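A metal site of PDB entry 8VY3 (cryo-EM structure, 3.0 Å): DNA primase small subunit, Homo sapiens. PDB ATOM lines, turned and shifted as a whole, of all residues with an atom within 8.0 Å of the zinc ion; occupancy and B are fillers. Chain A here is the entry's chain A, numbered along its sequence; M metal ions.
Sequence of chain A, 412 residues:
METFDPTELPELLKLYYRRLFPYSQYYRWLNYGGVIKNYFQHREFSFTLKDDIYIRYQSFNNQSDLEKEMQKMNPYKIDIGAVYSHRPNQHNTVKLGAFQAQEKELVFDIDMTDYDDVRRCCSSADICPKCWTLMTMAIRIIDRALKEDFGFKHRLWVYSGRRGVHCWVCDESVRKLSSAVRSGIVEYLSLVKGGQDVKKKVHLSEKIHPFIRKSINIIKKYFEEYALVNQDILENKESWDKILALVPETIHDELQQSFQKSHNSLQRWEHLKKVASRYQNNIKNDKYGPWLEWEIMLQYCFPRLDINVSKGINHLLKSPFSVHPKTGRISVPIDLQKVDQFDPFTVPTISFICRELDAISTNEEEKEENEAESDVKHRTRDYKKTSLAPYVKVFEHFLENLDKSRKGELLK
SG of Cys 122 lies close to O of Asp 126 (3.3 Å).
The side-chain sulfur of Cys 121 sits close to the side-chain amide nitrogen of Gln 231, at 3.6 Å.
The zinc ion is bound by SG of Cys 131, SG of Cys 128, SG of Cys 122 and SG of Cys 121.
The zinc ion has four donor atoms within binding distance.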
ATOM      1  N   MET A 112     -17.162 -10.813  -7.334  1.00  0.00           N
ATOM      2  CA  MET A 112     -16.288 -11.975  -7.430  1.00  0.00           C
ATOM      3  C   MET A 112     -17.037 -13.297  -7.486  1.00  0.00           C
ATOM      4  O   MET A 112     -16.500 -14.276  -8.010  1.00  0.00           O
ATOM      5  CB  MET A 112     -15.308 -12.011  -6.255  1.00  0.00           C
ATOM      6  CG  MET A 112     -13.850 -12.205  -6.623  1.00  0.00           C
ATOM      7  SD  MET A 112     -13.250 -11.058  -7.880  1.00  0.00           S
ATOM      8  CE  MET A 112     -12.348  -9.887  -6.866  1.00  0.00           C
ATOM      9  N   ARG A 119     -11.516 -18.537 -11.124  1.00  0.00           N
ATOM     10  CA  ARG A 119     -10.436 -18.341 -10.166  1.00  0.00           C
ATOM     11  C   ARG A 119      -9.879 -19.688  -9.716  1.00  0.00           C
ATOM     12  O   ARG A 119     -10.620 -20.570  -9.282  1.00  0.00           O
ATOM     13  CB  ARG A 119     -10.913 -17.550  -8.945  1.00  0.00           C
ATOM     14  CG  ARG A 119     -11.881 -16.426  -9.264  1.00  0.00           C
ATOM     15  CD  ARG A 119     -11.982 -15.452  -8.098  1.00  0.00           C
ATOM     16  NE  ARG A 119     -12.638 -16.051  -6.938  1.00  0.00           N
ATOM     17  CZ  ARG A 119     -13.927 -16.336  -6.869  1.00  0.00           C
ATOM     18  NH1 ARG A 119     -14.755 -16.083  -7.868  1.00  0.00           N
ATOM     19  NH2 ARG A 119     -14.402 -16.893  -5.758  1.00  0.00           N
ATOM     20  N   ARG A 120      -8.561 -19.821  -9.821  1.00  0.00           N
ATOM     21  CA  ARG A 120      -7.835 -20.990  -9.342  1.00  0.00           C
ATOM     22  C   ARG A 120      -6.751 -20.584  -8.344  1.00  0.00           C
ATOM     23  O   ARG A 120      -5.787 -21.321  -8.125  1.00  0.00           O
ATOM     24  CB  ARG A 120      -7.232 -21.766 -10.502  1.00  0.00           C
ATOM     25  CG  ARG A 120      -8.238 -22.170 -11.573  1.00  0.00           C
ATOM     26  CD  ARG A 120      -7.619 -23.104 -12.596  1.00  0.00           C
ATOM     27  NE  ARG A 120      -6.800 -24.147 -11.978  1.00  0.00           N
ATOM     28  CZ  ARG A 120      -5.734 -24.697 -12.543  1.00  0.00           C
ATOM     29  NH1 ARG A 120      -5.328 -24.332 -13.743  1.00  0.00           N
ATOM     30  NH2 ARG A 120      -5.070 -25.642 -11.886  1.00  0.00           N
ATOM     31  N   CYS A 121      -6.890 -19.402  -7.752  1.00  0.00           N
ATOM     32  CA  CYS A 121      -5.870 -18.840  -6.886  1.00  0.00           C
ATOM     33  C   CYS A 121      -6.335 -18.669  -5.442  1.00  0.00           C
ATOM     34  O   CYS A 121      -5.524 -18.829  -4.519  1.00  0.00           O
ATOM     35  CB  CYS A 121      -5.391 -17.498  -7.453  1.00  0.00           C
ATOM     36  SG  CYS A 121      -6.689 -16.275  -7.748  1.00  0.00           S
ATOM     37  N   CYS A 122      -7.597 -18.344  -5.219  1.00  0.00           N
ATOM     38  CA  CYS A 122      -8.149 -18.263  -3.877  1.00  0.00           C
ATOM     39  C   CYS A 122      -9.563 -18.820  -3.851  1.00  0.00           C
ATOM     40  O   CYS A 122     -10.215 -18.966  -4.895  1.00  0.00           O
ATOM     41  CB  CYS A 122      -8.135 -16.833  -3.326  1.00  0.00           C
ATOM     42  SG  CYS A 122      -8.406 -15.542  -4.559  1.00  0.00           S
ATOM     43  N   SER A 123     -10.042 -19.124  -2.648  1.00  0.00           N
ATOM     44  CA  SER A 123     -11.351 -19.727  -2.453  1.00  0.00           C
ATOM     45  C   SER A 123     -12.451 -18.673  -2.568  1.00  0.00           C
ATOM     46  O   SER A 123     -12.210 -17.510  -2.924  1.00  0.00           O
ATOM     47  CB  SER A 123     -11.416 -20.428  -1.107  1.00  0.00           C
ATOM     48  OG  SER A 123     -11.152 -19.524  -0.048  1.00  0.00           O
ATOM     49  N   ASP A 126     -11.909 -15.517  -0.302  1.00  0.00           N
ATOM     50  CA  ASP A 126     -10.613 -14.853  -0.344  1.00  0.00           C
ATOM     51  C   ASP A 126     -10.432 -14.118  -1.671  1.00  0.00           C
ATOM     52  O   ASP A 126     -10.900 -14.553  -2.724  1.00  0.00           O
ATOM     53  CB  ASP A 126      -9.480 -15.864  -0.142  1.00  0.00           C
ATOM     54  CG  ASP A 126      -9.633 -16.674   1.117  1.00  0.00           C
ATOM     55  OD1 ASP A 126      -9.806 -16.075   2.201  1.00  0.00           O
ATOM     56  OD2 ASP A 126      -9.586 -17.916   1.036  1.00  0.00           O
ATOM     57  N   ILE A 127      -9.742 -12.987  -1.592  1.00  0.00           N
ATOM     58  CA  ILE A 127      -9.312 -12.238  -2.773  1.00  0.00           C
ATOM     59  C   ILE A 127      -7.816 -11.980  -2.632  1.00  0.00           C
ATOM     60  O   ILE A 127      -7.263 -11.973  -1.539  1.00  0.00           O
ATOM     61  CB  ILE A 127     -10.082 -10.909  -2.952  1.00  0.00           C
ATOM     62  CG1 ILE A 127      -9.432  -9.782  -2.152  1.00  0.00           C
ATOM     63  CG2 ILE A 127     -11.541 -11.066  -2.551  1.00  0.00           C
ATOM     64  CD1 ILE A 127      -9.934  -8.400  -2.517  1.00  0.00           C
ATOM     65  N   CYS A 128      -7.166 -11.765  -3.773  1.00  0.00           N
ATOM     66  CA  CYS A 128      -5.721 -11.534  -3.795  1.00  0.00           C
ATOM     67  C   CYS A 128      -5.413 -10.631  -4.974  1.00  0.00           C
ATOM     68  O   CYS A 128      -6.180 -10.569  -5.941  1.00  0.00           O
ATOM     69  CB  CYS A 128      -4.941 -12.851  -3.868  1.00  0.00           C
ATOM     70  SG  CYS A 128      -5.057 -13.719  -5.455  1.00  0.00           S
ATOM     71  N   PRO A 129      -4.291  -9.898  -4.931  1.00  0.00           N
ATOM     72  CA  PRO A 129      -3.997  -8.929  -6.002  1.00  0.00           C
ATOM     73  C   PRO A 129      -3.907  -9.533  -7.397  1.00  0.00           C
ATOM     74  O   PRO A 129      -4.252  -8.867  -8.369  1.00  0.00           O
ATOM     75  CB  PRO A 129      -2.659  -8.325  -5.553  1.00  0.00           C
ATOM     76  CG  PRO A 129      -2.671  -8.464  -4.074  1.00  0.00           C
ATOM     77  CD  PRO A 129      -3.328  -9.796  -3.823  1.00  0.00           C
ATOM     78  N   LYS A 130      -3.452 -10.785  -7.511  1.00  0.00           N
ATOM     79  CA  LYS A 130      -3.223 -11.356  -8.835  1.00  0.00           C
ATOM     80  C   LYS A 130      -4.508 -11.820  -9.513  1.00  0.00           C
ATOM     81  O   LYS A 130      -4.454 -12.255 -10.673  1.00  0.00           O
ATOM     82  CB  LYS A 130      -2.208 -12.501  -8.746  1.00  0.00           C
ATOM     83  CG  LYS A 130      -2.748 -13.816  -8.229  1.00  0.00           C
ATOM     84  CD  LYS A 130      -1.592 -14.688  -7.765  1.00  0.00           C
ATOM     85  CE  LYS A 130      -2.014 -15.685  -6.707  1.00  0.00           C
ATOM     86  NZ  LYS A 130      -2.170 -17.054  -7.281  1.00  0.00           N
ATOM     87  N   CYS A 131      -5.649 -11.764  -8.824  1.00  0.00           N
ATOM     88  CA  CYS A 131      -6.931 -11.977  -9.483  1.00  0.00           C
ATOM     89  C   CYS A 131      -7.777 -10.707  -9.529  1.00  0.00           C
ATOM     90  O   CYS A 131      -8.752 -10.664 -10.289  1.00  0.00           O
ATOM     91  CB  CYS A 131      -7.739 -13.089  -8.799  1.00  0.00           C
ATOM     92  SG  CYS A 131      -8.217 -12.755  -7.099  1.00  0.00           S
ATOM     93  N   TRP A 132      -7.433  -9.682  -8.751  1.00  0.00           N
ATOM     94  CA  TRP A 132      -8.190  -8.428  -8.751  1.00  0.00           C
ATOM     95  C   TRP A 132      -8.180  -7.741 -10.111  1.00  0.00           C
ATOM     96  O   TRP A 132      -9.015  -6.859 -10.339  1.00  0.00           O
ATOM     97  CB  TRP A 132      -7.644  -7.480  -7.685  1.00  0.00           C
ATOM     98  CG  TRP A 132      -8.395  -6.181  -7.586  1.00  0.00           C
ATOM     99  CD1 TRP A 132      -7.968  -4.965  -8.047  1.00  0.00           C
ATOM    100  CD2 TRP A 132      -9.688  -5.976  -7.012  1.00  0.00           C
ATOM    101  NE1 TRP A 132      -8.923  -4.018  -7.787  1.00  0.00           N
ATOM    102  CE2 TRP A 132      -9.986  -4.606  -7.151  1.00  0.00           C
ATOM    103  CE3 TRP A 132     -10.618  -6.811  -6.393  1.00  0.00           C
ATOM    104  CZ2 TRP A 132     -11.185  -4.054  -6.698  1.00  0.00           C
ATOM    105  CZ3 TRP A 132     -11.805  -6.254  -5.937  1.00  0.00           C
ATOM    106  CH2 TRP A 132     -12.072  -4.888  -6.097  1.00  0.00           C
ATOM    107  N   TYR A 226      -2.211 -12.381 -16.927  1.00  0.00           N
ATOM    108  CA  TYR A 226      -3.069 -12.920 -15.886  1.00  0.00           C
ATOM    109  C   TYR A 226      -3.397 -14.398 -16.115  1.00  0.00           C
ATOM    110  O   TYR A 226      -3.186 -15.230 -15.217  1.00  0.00           O
ATOM    111  CB  TYR A 226      -4.362 -12.097 -15.804  1.00  0.00           C
ATOM    112  CG  TYR A 226      -5.489 -12.749 -15.040  1.00  0.00           C
ATOM    113  CD1 TYR A 226      -5.295 -13.200 -13.742  1.00  0.00           C
ATOM    114  CD2 TYR A 226      -6.737 -12.919 -15.614  1.00  0.00           C
ATOM    115  CE1 TYR A 226      -6.315 -13.804 -13.033  1.00  0.00           C
ATOM    116  CE2 TYR A 226      -7.762 -13.523 -14.917  1.00  0.00           C
ATOM    117  CZ  TYR A 226      -7.550 -13.960 -13.627  1.00  0.00           C
ATOM    118  OH  TYR A 226      -8.571 -14.555 -12.932  1.00  0.00           O
ATOM    119  N   GLN A 231      -2.391 -17.693 -13.539  1.00  0.00           N
ATOM    120  CA  GLN A 231      -3.378 -18.731 -13.254  1.00  0.00           C
ATOM    121  C   GLN A 231      -2.943 -20.115 -13.709  1.00  0.00           C
ATOM    122  O   GLN A 231      -3.317 -21.108 -13.074  1.00  0.00           O
ATOM    123  CB  GLN A 231      -4.717 -18.383 -13.917  1.00  0.00           C
ATOM    124  CG  GLN A 231      -5.655 -17.475 -13.093  1.00  0.00           C
ATOM    125  CD  GLN A 231      -6.083 -18.057 -11.740  1.00  0.00           C
ATOM    126  OE1 GLN A 231      -5.532 -19.037 -11.243  1.00  0.00           O
ATOM    127  NE2 GLN A 231      -7.091 -17.427 -11.146  1.00  0.00           N
HETATM  128 ZN    ZN M   1      -7.080 -14.571  -6.209  1.00  0.00          ZN
